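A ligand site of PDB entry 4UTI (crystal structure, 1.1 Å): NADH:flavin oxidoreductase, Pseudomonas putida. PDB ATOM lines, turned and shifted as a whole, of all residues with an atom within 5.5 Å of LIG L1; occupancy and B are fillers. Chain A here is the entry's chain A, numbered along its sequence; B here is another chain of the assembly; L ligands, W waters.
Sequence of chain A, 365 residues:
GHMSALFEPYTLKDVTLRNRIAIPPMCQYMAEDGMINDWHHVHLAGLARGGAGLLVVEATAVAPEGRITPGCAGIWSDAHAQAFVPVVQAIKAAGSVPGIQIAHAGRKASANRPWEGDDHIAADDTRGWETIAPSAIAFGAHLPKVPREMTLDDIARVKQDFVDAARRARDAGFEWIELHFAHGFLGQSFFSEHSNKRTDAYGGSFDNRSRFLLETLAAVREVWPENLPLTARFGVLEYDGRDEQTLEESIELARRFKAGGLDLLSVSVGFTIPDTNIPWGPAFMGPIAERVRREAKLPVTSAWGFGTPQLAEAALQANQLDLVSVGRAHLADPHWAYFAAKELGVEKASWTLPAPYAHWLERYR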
ATOM      1  N   PRO A  24      18.629  18.333 -22.173  1.00  0.00           N
ATOM      2  CA  PRO A  24      17.280  18.255 -22.734  1.00  0.00           C
ATOM      3  C   PRO A  24      17.146  19.271 -23.853  1.00  0.00           C
ATOM      4  O   PRO A  24      17.936  20.205 -23.968  1.00  0.00           O
ATOM      5  CB  PRO A  24      16.406  18.618 -21.535  1.00  0.00           C
ATOM      6  CG  PRO A  24      17.261  19.605 -20.772  1.00  0.00           C
ATOM      7  CD  PRO A  24      18.648  19.095 -20.914  1.00  0.00           C
ATOM      8  N   PRO A  25      16.101  19.103 -24.673  1.00  0.00           N
ATOM      9  CA  PRO A  25      15.860  20.062 -25.745  1.00  0.00           C
ATOM     10  C   PRO A  25      15.702  21.474 -25.181  1.00  0.00           C
ATOM     11  O   PRO A  25      14.973  21.682 -24.232  1.00  0.00           O
ATOM     12  CB  PRO A  25      14.557  19.542 -26.390  1.00  0.00           C
ATOM     13  CG  PRO A  25      13.918  18.694 -25.301  1.00  0.00           C
ATOM     14  CD  PRO A  25      15.065  18.059 -24.605  1.00  0.00           C
ATOM     15  N   MET A  26      16.386  22.424 -25.807  1.00  0.00           N
ATOM     16  CA  MET A  26      16.261  23.839 -25.435  1.00  0.00           C
ATOM     17  C   MET A  26      16.218  24.712 -26.684  1.00  0.00           C
ATOM     18  O   MET A  26      17.267  24.989 -27.309  1.00  0.00           O
ATOM     19  CB  MET A  26      17.402  24.297 -24.511  1.00  0.00           C
ATOM     20  CG  MET A  26      17.261  23.741 -23.115  1.00  0.00           C
ATOM     21  SD  MET A  26      18.600  24.300 -22.003  1.00  0.00           S
ATOM     22  CE  MET A  26      19.934  23.336 -22.657  1.00  0.00           C
ATOM     23  N   CYS A  27      15.027  25.167 -27.013  1.00  0.00           N
ATOM     24  CA  CYS A  27      14.835  26.117 -28.095  1.00  0.00           C
ATOM     25  C   CYS A  27      15.807  27.289 -28.022  1.00  0.00           C
ATOM     26  O   CYS A  27      16.008  27.878 -26.952  1.00  0.00           O
ATOM     27  CB  CYS A  27      13.419  26.660 -28.076  1.00  0.00           C
ATOM     28  SG  CYS A  27      12.164  25.530 -28.699  1.00  0.00           S
ATOM     29  N   GLN A  28      16.347  27.630 -29.186  1.00  0.00           N
ATOM     30  CA  GLN A  28      17.278  28.734 -29.328  1.00  0.00           C
ATOM     31  C   GLN A  28      16.690  29.944 -30.043  1.00  0.00           C
ATOM     32  O   GLN A  28      17.228  31.041 -29.937  1.00  0.00           O
ATOM     33  CB  GLN A  28      18.516  28.248 -30.081  1.00  0.00           C
ATOM     34  CG  GLN A  28      19.279  27.162 -29.339  1.00  0.00           C
ATOM     35  CD  GLN A  28      19.840  27.652 -28.046  1.00  0.00           C
ATOM     36  OE1 GLN A  28      20.803  28.415 -28.018  1.00  0.00           O
ATOM     37  NE2 GLN A  28      19.238  27.222 -26.944  1.00  0.00           N
ATOM     38  N   TYR A  29      15.603  29.742 -30.779  1.00  0.00           N
ATOM     39  CA  TYR A  29      14.906  30.839 -31.444  1.00  0.00           C
ATOM     40  C   TYR A  29      15.781  31.570 -32.466  1.00  0.00           C
ATOM     41  O   TYR A  29      15.567  32.763 -32.725  1.00  0.00           O
ATOM     42  CB  TYR A  29      14.285  31.808 -30.432  1.00  0.00           C
ATOM     43  CG  TYR A  29      13.482  31.121 -29.354  1.00  0.00           C
ATOM     44  CD1 TYR A  29      12.144  30.805 -29.544  1.00  0.00           C
ATOM     45  CD2 TYR A  29      14.073  30.742 -28.158  1.00  0.00           C
ATOM     46  CE1 TYR A  29      11.412  30.150 -28.561  1.00  0.00           C
ATOM     47  CE2 TYR A  29      13.348  30.079 -27.174  1.00  0.00           C
ATOM     48  CZ  TYR A  29      12.011  29.804 -27.377  1.00  0.00           C
ATOM     49  OH  TYR A  29      11.322  29.148 -26.385  1.00  0.00           O
ATOM     50  N   GLU A  58      16.766  20.859 -29.614  1.00  0.00           N
ATOM     51  CA  GLU A  58      15.538  21.607 -29.366  1.00  0.00           C
ATOM     52  C   GLU A  58      14.335  21.154 -30.178  1.00  0.00           C
ATOM     53  O   GLU A  58      14.468  20.626 -31.290  1.00  0.00           O
ATOM     54  CB  GLU A  58      15.794  23.081 -29.708  1.00  0.00           C
ATOM     55  CG  GLU A  58      16.108  23.366 -31.194  1.00  0.00           C
ATOM     56  CD  GLU A  58      16.724  24.750 -31.364  1.00  0.00           C
ATOM     57  OE1 GLU A  58      15.960  25.743 -31.446  1.00  0.00           O
ATOM     58  OE2 GLU A  58      17.965  24.839 -31.374  1.00  0.00           O
ATOM     59  N   ALA A  59      13.151  21.456 -29.641  1.00  0.00           N
ATOM     60  CA  ALA A  59      11.894  21.234 -30.352  1.00  0.00           C
ATOM     61  C   ALA A  59      12.002  21.673 -31.797  1.00  0.00           C
ATOM     62  O   ALA A  59      12.163  22.870 -32.094  1.00  0.00           O
ATOM     63  CB  ALA A  59      10.771  21.987 -29.674  1.00  0.00           C
ATOM     64  N   GLN A 101      14.332  16.331 -30.586  1.00  0.00           N
ATOM     65  CA  GLN A 101      12.923  16.359 -30.202  1.00  0.00           C
ATOM     66  C   GLN A 101      12.126  16.889 -31.388  1.00  0.00           C
ATOM     67  O   GLN A 101      12.367  18.014 -31.830  1.00  0.00           O
ATOM     68  CB  GLN A 101      12.735  17.267 -28.982  1.00  0.00           C
ATOM     69  CG  GLN A 101      11.318  17.228 -28.471  1.00  0.00           C
ATOM     70  CD  GLN A 101      11.054  18.260 -27.411  1.00  0.00           C
ATOM     71  OE1 GLN A 101      11.186  19.445 -27.696  1.00  0.00           O
ATOM     72  NE2 GLN A 101      10.653  17.844 -26.223  1.00  0.00           N
ATOM     73  N   GLU A 178      12.909  12.000 -29.696  1.00  0.00           N
ATOM     74  CA  GLU A 178      11.931  12.311 -28.651  1.00  0.00           C
ATOM     75  C   GLU A 178      10.707  12.960 -29.287  1.00  0.00           C
ATOM     76  O   GLU A 178      10.816  14.018 -29.902  1.00  0.00           O
ATOM     77  CB  GLU A 178      12.547  13.231 -27.607  1.00  0.00           C
ATOM     78  CG  GLU A 178      11.625  13.454 -26.405  1.00  0.00           C
ATOM     79  CD  GLU A 178      12.255  14.386 -25.382  1.00  0.00           C
ATOM     80  OE1 GLU A 178      13.205  13.964 -24.701  1.00  0.00           O
ATOM     81  OE2 GLU A 178      11.826  15.529 -25.242  1.00  0.00           O
ATOM     82  N   HIS A 180       7.547  15.158 -28.938  1.00  0.00           N
ATOM     83  CA  HIS A 180       7.168  16.198 -27.987  1.00  0.00           C
ATOM     84  C   HIS A 180       5.678  16.183 -27.727  1.00  0.00           C
ATOM     85  O   HIS A 180       4.895  16.885 -28.386  1.00  0.00           O
ATOM     86  CB  HIS A 180       7.587  17.554 -28.482  1.00  0.00           C
ATOM     87  CG  HIS A 180       7.585  18.585 -27.406  1.00  0.00           C
ATOM     88  ND1 HIS A 180       7.064  18.351 -26.142  1.00  0.00           N
ATOM     89  CD2 HIS A 180       8.134  19.824 -27.382  1.00  0.00           C
ATOM     90  CE1 HIS A 180       7.299  19.416 -25.395  1.00  0.00           C
ATOM     91  NE2 HIS A 180       7.945  20.323 -26.127  1.00  0.00           N
ATOM     92  N   HIS A 183       3.977  19.912 -22.527  1.00  0.00           N
ATOM     93  CA  HIS A 183       4.096  21.369 -22.463  1.00  0.00           C
ATOM     94  C   HIS A 183       2.995  22.098 -23.209  1.00  0.00           C
ATOM     95  O   HIS A 183       3.158  23.234 -23.631  1.00  0.00           O
ATOM     96  CB  HIS A 183       5.502  21.829 -22.880  1.00  0.00           C
ATOM     97  CG  HIS A 183       6.596  21.225 -22.024  1.00  0.00           C
ATOM     98  ND1 HIS A 183       7.925  21.319 -22.347  1.00  0.00           N
ATOM     99  CD2 HIS A 183       6.537  20.524 -20.869  1.00  0.00           C
ATOM    100  CE1 HIS A 183       8.644  20.698 -21.423  1.00  0.00           C
ATOM    101  NE2 HIS A 183       7.825  20.203 -20.513  1.00  0.00           N
ATOM    102  N   ARG A 233       8.413  12.951 -24.618  1.00  0.00           N
ATOM    103  CA  ARG A 233       8.229  13.819 -23.454  1.00  0.00           C
ATOM    104  C   ARG A 233       6.730  13.981 -23.270  1.00  0.00           C
ATOM    105  O   ARG A 233       5.995  14.200 -24.250  1.00  0.00           O
ATOM    106  CB  ARG A 233       8.935  15.176 -23.644  1.00  0.00           C
ATOM    107  CG  ARG A 233       9.110  15.925 -22.306  1.00  0.00           C
ATOM    108  CD  ARG A 233      10.066  17.096 -22.404  1.00  0.00           C
ATOM    109  NE  ARG A 233      10.736  17.303 -21.129  1.00  0.00           N
ATOM    110  CZ  ARG A 233      11.652  18.242 -20.895  1.00  0.00           C
ATOM    111  NH1 ARG A 233      11.907  19.170 -21.792  1.00  0.00           N
ATOM    112  NH2 ARG A 233      12.291  18.207 -19.719  1.00  0.00           N
ATOM    113  N   ALA A 303      13.570  16.825 -15.387  1.00  0.00           N
ATOM    114  CA  ALA A 303      14.331  18.056 -15.366  1.00  0.00           C
ATOM    115  C   ALA A 303      13.689  19.018 -14.373  1.00  0.00           C
ATOM    116  O   ALA A 303      12.590  18.780 -13.891  1.00  0.00           O
ATOM    117  CB  ALA A 303      14.370  18.695 -16.747  1.00  0.00           C
ATOM    118  N   TRP A 304      14.447  20.072 -14.106  1.00  0.00           N
ATOM    119  CA  TRP A 304      14.135  21.271 -13.340  1.00  0.00           C
ATOM    120  C   TRP A 304      14.954  21.275 -12.060  1.00  0.00           C
ATOM    121  O   TRP A 304      14.591  20.623 -11.044  1.00  0.00           O
ATOM    122  CB  TRP A 304      12.663  21.520 -13.054  1.00  0.00           C
ATOM    123  CG  TRP A 304      12.512  22.902 -12.407  1.00  0.00           C
ATOM    124  CD1 TRP A 304      12.743  23.264 -11.087  1.00  0.00           C
ATOM    125  CD2 TRP A 304      12.129  24.086 -13.084  1.00  0.00           C
ATOM    126  NE1 TRP A 304      12.513  24.607 -10.928  1.00  0.00           N
ATOM    127  CE2 TRP A 304      12.139  25.134 -12.141  1.00  0.00           C
ATOM    128  CE3 TRP A 304      11.758  24.362 -14.406  1.00  0.00           C
ATOM    129  CZ2 TRP A 304      11.794  26.445 -12.478  1.00  0.00           C
ATOM    130  CZ3 TRP A 304      11.427  25.659 -14.733  1.00  0.00           C
ATOM    131  CH2 TRP A 304      11.444  26.686 -13.778  1.00  0.00           C
ATOM    132  N   GLY A 305      16.057  22.013 -12.093  1.00  0.00           N
ATOM    133  CA  GLY A 305      16.894  22.190 -10.929  1.00  0.00           C
ATOM    134  C   GLY A 305      17.969  21.128 -10.686  1.00  0.00           C
ATOM    135  O   GLY A 305      18.537  21.104  -9.580  1.00  0.00           O
ATOM    136  N   PHE A 306      18.255  20.261 -11.641  1.00  0.00           N
ATOM    137  CA  PHE A 306      19.282  19.235 -11.410  1.00  0.00           C
ATOM    138  C   PHE A 306      20.724  19.697 -11.707  1.00  0.00           C
ATOM    139  O   PHE A 306      21.657  18.887 -11.644  1.00  0.00           O
ATOM    140  CB  PHE A 306      18.954  17.971 -12.199  1.00  0.00           C
ATOM    141  CG  PHE A 306      17.766  17.215 -11.671  1.00  0.00           C
ATOM    142  CD1 PHE A 306      17.880  16.429 -10.531  1.00  0.00           C
ATOM    143  CD2 PHE A 306      16.533  17.267 -12.326  1.00  0.00           C
ATOM    144  CE1 PHE A 306      16.785  15.714 -10.059  1.00  0.00           C
ATOM    145  CE2 PHE A 306      15.439  16.566 -11.854  1.00  0.00           C
ATOM    146  CZ  PHE A 306      15.568  15.780 -10.705  1.00  0.00           C
ATOM    147  N   GLY A 307      20.910  20.989 -11.962  1.00  0.00           N
ATOM    148  CA  GLY A 307      22.232  21.566 -12.126  1.00  0.00           C
ATOM    149  C   GLY A 307      23.072  21.575 -10.857  1.00  0.00           C
ATOM    150  O   GLY A 307      24.251  21.903 -10.926  1.00  0.00           O
ATOM    151  N   SER A 325      18.323  15.171 -16.665  1.00  0.00           N
ATOM    152  CA  SER A 325      18.340  16.227 -17.670  1.00  0.00           C
ATOM    153  C   SER A 325      18.711  17.550 -16.997  1.00  0.00           C
ATOM    154  O   SER A 325      18.083  17.949 -16.016  1.00  0.00           O
ATOM    155  CB  SER A 325      16.996  16.307 -18.365  1.00  0.00           C
ATOM    156  OG  SER A 325      16.757  15.154 -19.155  1.00  0.00           O
ATOM    157  N   VAL A 326      19.726  18.211 -17.554  1.00  0.00           N
ATOM    158  CA  VAL A 326      20.296  19.437 -17.017  1.00  0.00           C
ATOM    159  C   VAL A 326      20.319  20.475 -18.141  1.00  0.00           C
ATOM    160  O   VAL A 326      21.094  20.393 -19.092  1.00  0.00           O
ATOM    161  CB  VAL A 326      21.704  19.186 -16.449  1.00  0.00           C
ATOM    162  CG1 VAL A 326      22.291  20.496 -15.930  1.00  0.00           C
ATOM    163  CG2 VAL A 326      21.673  18.138 -15.365  1.00  0.00           C
ATOM    164  N   GLY A 327      19.423  21.455 -18.029  1.00  0.00           N
ATOM    165  CA  GLY A 327      19.203  22.436 -19.093  1.00  0.00           C
ATOM    166  C   GLY A 327      19.928  23.756 -18.878  1.00  0.00           C
ATOM    167  O   GLY A 327      21.005  23.995 -19.440  1.00  0.00           O
ATOM    168  N   ARG A 328      19.337  24.643 -18.071  1.00  0.00           N
ATOM    169  CA  ARG A 328      19.871  26.000 -17.926  1.00  0.00           C
ATOM    170  C   ARG A 328      21.316  26.038 -17.453  1.00  0.00           C
ATOM    171  O   ARG A 328      22.071  26.919 -17.874  1.00  0.00           O
ATOM    172  CB  ARG A 328      18.946  26.855 -17.049  1.00  0.00           C
ATOM    173  CG  ARG A 328      17.706  27.290 -17.797  1.00  0.00           C
ATOM    174  CD  ARG A 328      16.643  27.853 -16.903  1.00  0.00           C
ATOM    175  NE  ARG A 328      16.087  26.819 -16.041  1.00  0.00           N
ATOM    176  CZ  ARG A 328      15.182  27.053 -15.111  1.00  0.00           C
ATOM    177  NH1 ARG A 328      14.721  28.279 -14.927  1.00  0.00           N
ATOM    178  NH2 ARG A 328      14.759  26.039 -14.364  1.00  0.00           N
ATOM    179  N   ALA A 329      21.731  25.087 -16.616  1.00  0.00           N
ATOM    180  CA  ALA A 329      23.104  25.083 -16.169  1.00  0.00           C
ATOM    181  C   ALA A 329      24.079  24.954 -17.339  1.00  0.00           C
ATOM    182  O   ALA A 329      25.216  25.417 -17.249  1.00  0.00           O
ATOM    183  CB  ALA A 329      23.340  24.007 -15.137  1.00  0.00           C
ATOM    184  N   LEU A 331      23.438  26.252 -20.411  1.00  0.00           N
ATOM    185  CA  LEU A 331      23.492  27.559 -21.036  1.00  0.00           C
ATOM    186  C   LEU A 331      24.485  28.455 -20.288  1.00  0.00           C
ATOM    187  O   LEU A 331      25.268  29.182 -20.907  1.00  0.00           O
ATOM    188  CB  LEU A 331      22.108  28.210 -21.068  1.00  0.00           C
ATOM    189  CG  LEU A 331      20.992  27.373 -21.688  1.00  0.00           C
ATOM    190  CD1 LEU A 331      19.691  28.171 -21.713  1.00  0.00           C
ATOM    191  CD2 LEU A 331      21.343  26.904 -23.100  1.00  0.00           C
ATOM    192  N   PRO B 356      19.785  34.099 -26.532  1.00  0.00           N
ATOM    193  CA  PRO B 356      19.277  32.736 -26.325  1.00  0.00           C
ATOM    194  C   PRO B 356      19.774  32.070 -25.042  1.00  0.00           C
ATOM    195  O   PRO B 356      19.231  31.028 -24.661  1.00  0.00           O
ATOM    196  CB  PRO B 356      19.754  31.972 -27.563  1.00  0.00           C
ATOM    197  CG  PRO B 356      19.984  33.046 -28.603  1.00  0.00           C
ATOM    198  CD  PRO B 356      20.472  34.238 -27.831  1.00  0.00           C
ATOM    199  N   TRP B 360      17.304  33.518 -20.103  1.00  0.00           N
ATOM    200  CA  TRP B 360      16.916  32.439 -19.190  1.00  0.00           C
ATOM    201  C   TRP B 360      17.713  32.422 -17.908  1.00  0.00           C
ATOM    202  O   TRP B 360      17.388  31.691 -16.975  1.00  0.00           O
ATOM    203  CB  TRP B 360      17.103  31.099 -19.901  1.00  0.00           C
ATOM    204  CG  TRP B 360      16.440  31.116 -21.216  1.00  0.00           C
ATOM    205  CD1 TRP B 360      17.041  31.194 -22.438  1.00  0.00           C
ATOM    206  CD2 TRP B 360      15.037  31.146 -21.454  1.00  0.00           C
ATOM    207  NE1 TRP B 360      16.095  31.271 -23.421  1.00  0.00           N
ATOM    208  CE2 TRP B 360      14.856  31.223 -22.853  1.00  0.00           C
ATOM    209  CE3 TRP B 360      13.915  31.089 -20.616  1.00  0.00           C
ATOM    210  CZ2 TRP B 360      13.588  31.234 -23.423  1.00  0.00           C
ATOM    211  CZ3 TRP B 360      12.676  31.112 -21.188  1.00  0.00           C
ATOM    212  CH2 TRP B 360      12.516  31.183 -22.576  1.00  0.00           C
HETATM  213  N1  LIG L   1      11.550  21.708 -23.229  1.00  0.00           N
HETATM  214  C1  LIG L   1      11.153  20.977 -24.293  1.00  0.00           C
HETATM  215  O1  LIG L   1      10.530  19.792 -24.130  1.00  0.00           O
HETATM  216  N2  LIG L   1      11.509  21.367 -25.618  1.00  0.00           N
HETATM  217  C2  LIG L   1      12.177  22.515 -25.950  1.00  0.00           C
HETATM  218  O2  LIG L   1      12.628  22.747 -27.092  1.00  0.00           O
HETATM  219  C3  LIG L   1      12.402  23.343 -24.740  1.00  0.00           C
HETATM  220  N3  LIG L   1      13.045  24.563 -25.058  1.00  0.00           N
HETATM  221  C4  LIG L   1      13.528  25.260 -23.862  1.00  0.00           C
HETATM  222  C5  LIG L   1      14.385  26.354 -24.162  1.00  0.00           C
HETATM  223  C6  LIG L   1      15.075  26.961 -23.092  1.00  0.00           C
HETATM  224  C7  LIG L   1      16.014  28.135 -23.331  1.00  0.00           C
HETATM  225  C8  LIG L   1      14.810  26.536 -21.716  1.00  0.00           C
HETATM  226  C9  LIG L   1      15.466  27.148 -20.535  1.00  0.00           C
HETATM  227  C10 LIG L   1      13.966  25.449 -21.506  1.00  0.00           C
HETATM  228  C11 LIG L   1      13.407  24.769 -22.612  1.00  0.00           C
HETATM  229  N4  LIG L   1      12.637  23.576 -22.365  1.00  0.00           N
HETATM  230  C12 LIG L   1      12.204  22.846 -23.509  1.00  0.00           C
HETATM  231  C13 LIG L   1      12.647  22.912 -21.003  1.00  0.00           C
HETATM  232  C14 LIG L   1      14.010  22.319 -20.636  1.00  0.00           C
HETATM  233  O3  LIG L   1      14.117  21.179 -21.543  1.00  0.00           O
HETATM  234  C15 LIG L   1      14.050  21.856 -19.161  1.00  0.00           C
HETATM  235  O4  LIG L   1      12.962  20.886 -18.927  1.00  0.00           O
HETATM  236  C16 LIG L   1      13.839  23.028 -18.184  1.00  0.00           C
HETATM  237  O5  LIG L   1      14.777  24.051 -18.610  1.00  0.00           O
HETATM  238  C17 LIG L   1      14.157  22.617 -16.729  1.00  0.00           C
HETATM  239  O6  LIG L   1      15.506  22.131 -16.611  1.00  0.00           O
HETATM  240  P1  LIG L   1      16.668  23.054 -15.968  1.00  0.00           P
HETATM  241  O7  LIG L   1      16.869  24.245 -16.888  1.00  0.00           O
HETATM  242  O8  LIG L   1      16.111  23.507 -14.582  1.00  0.00           O
HETATM  243  O9  LIG L   1      17.859  22.130 -15.890  1.00  0.00           O
HETATM  244  C1  LG2 L   2       9.227  23.899 -24.570  1.00  0.00           C
HETATM  245  C2  LG2 L   2       9.682  24.732 -25.584  1.00  0.00           C
HETATM  246  C3  LG2 L   2      10.327  25.945 -25.248  1.00  0.00           C
HETATM  247  C4  LG2 L   2      10.490  26.342 -23.880  1.00  0.00           C
HETATM  248  C5  LG2 L   2      11.128  27.538 -23.492  1.00  0.00           C
HETATM  249  C6  LG2 L   2      11.243  27.809 -22.122  1.00  0.00           C
HETATM  250  C7  LG2 L   2      10.743  26.931 -21.154  1.00  0.00           C
HETATM  251  C8  LG2 L   2      10.113  25.755 -21.554  1.00  0.00           C
HETATM  252  C9  LG2 L   2      10.004  25.462 -22.922  1.00  0.00           C
HETATM  253  O1  LG2 L   2       8.653  22.769 -24.654  1.00  0.00           O
HETATM  254  O2  LG2 L   2       9.366  24.243 -23.247  1.00  0.00           O
HETATM  255  O   HOH W   1      17.711  25.148 -13.005  1.00  0.00           O
HETATM  256  O   HOH W   2      10.549  22.012 -18.419  1.00  0.00           O
HETATM  257  O   HOH W   3      17.271  20.001 -14.391  1.00  0.00           O
HETATM  258  O   HOH W   4      12.774  26.204 -17.876  1.00  0.00           O
HETATM  259  O   HOH W   5      20.208  23.283 -15.048  1.00  0.00           O
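Merely in contact with LIG L1: Pro 24, Met 26, Glu 58, His 183, Ala 303, Val 326 and Trp 360 of chain B.
Hydrophobic or aromatic side chains that line LIG L1: Pro 24, Pro 25, Met 26, Ala 59, His 180, His 183, Ala 303, Trp 304 and Trp 360 of chain B.
Within 4 Å of LIG L1: Pro 24, Pro 25, Met 26, Cys 27, Glu 58, Ala 59, Gln 101, His 180, His 183, Arg 233, Ala 303, Trp 304, Gly 305, Val 326, Gly 327, Arg 328 and Trp 360 of chain B.
The nearest printed residue that does not touch LIG L1 is Leu 331 (4.02 Å).
Water W5 lies within hydrogen-bond range of O9 of LIG L1 (2.7 Å), N of Ala 329 (2.8 Å) and N of Arg 328 (3.4 Å).
Water W1 lies within hydrogen-bond range of O8 of LIG L1 (2.8 Å) and NH2 of Arg 328 (3.4 Å).
N2 of LIG L1 lies close to O1 of LG2 L2 (3.3 Å).
The side-chain amide nitrogen (NE2) of Gln 101 lies within hydrogen-bond range of the side-chain carboxylate (OE2) of Glu 178 (2.8 Å).
NE1 of Trp 360 of chain B lies close to O of Pro 356 of chain B (3.4 Å).
The backbone NH of Ala 59 sits close to the side-chain amide oxygen of Gln 101 (3.4 Å).
The side-chain carboxylate (OE1) of Glu 58 is in hydrogen-bond range of the backbone NH (N) of Gln 28, 3.0 Å away.
NE2 of Gln 28 sits at hydrogen-bond distance from O of Met 26, 3.0 Å away.
A nitrogen (N2) of LIG L1 is in hydrogen-bond range of the side-chain amide oxygen of Gln 101, at 2.8 Å.
The backbone NH (N) of Trp 304 sits at hydrogen-bond distance from an oxygen (O6) of LIG L1, 3.4 Å away.
An oxygen (O1) of LG2 L2 lies within hydrogen-bond range of a ring nitrogen (ND1) of His 183, at 2.8 Å.
O8 of LIG L1 is in hydrogen-bond range of N of Gly 305, 2.9 Å away.
N of Cys 27 lies within hydrogen-bond range of N3 of LIG L1 (2.8 Å).
An oxygen (O7) of LIG L1 lies within salt-bridge range of the guanidinium group (NE) of Arg 328, 2.8 Å away.
An oxygen (O1) of LIG L1 lies within hydrogen-bond range of the guanidinium group (NH1) of Arg 233, 2.8 Å away.
An oxygen (O9) of LIG L1 is in hydrogen-bond range of the backbone NH (N) of Gly 327 (2.7 Å).
The side-chain sulfur of Cys 27 sits at hydrogen-bond distance from an oxygen (O2) of LIG L1, 3.2 Å away.
NE2 of His 180 sits at hydrogen-bond distance from O1 of LIG L1 (3.3 Å).
O of Pro 25 sits at hydrogen-bond distance from O3 of LIG L1, 2.9 Å away.
O1 of LG2 L2 is in hydrogen-bond range of NE2 of His 180 (2.9 Å).
The backbone NH of Ala 59 sits at hydrogen-bond distance from an oxygen (O2) of LIG L1, 2.9 Å away.
The backbone NH (N) of Arg 328 is in hydrogen-bond range of an oxygen (O7) of LIG L1 (2.8 Å).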
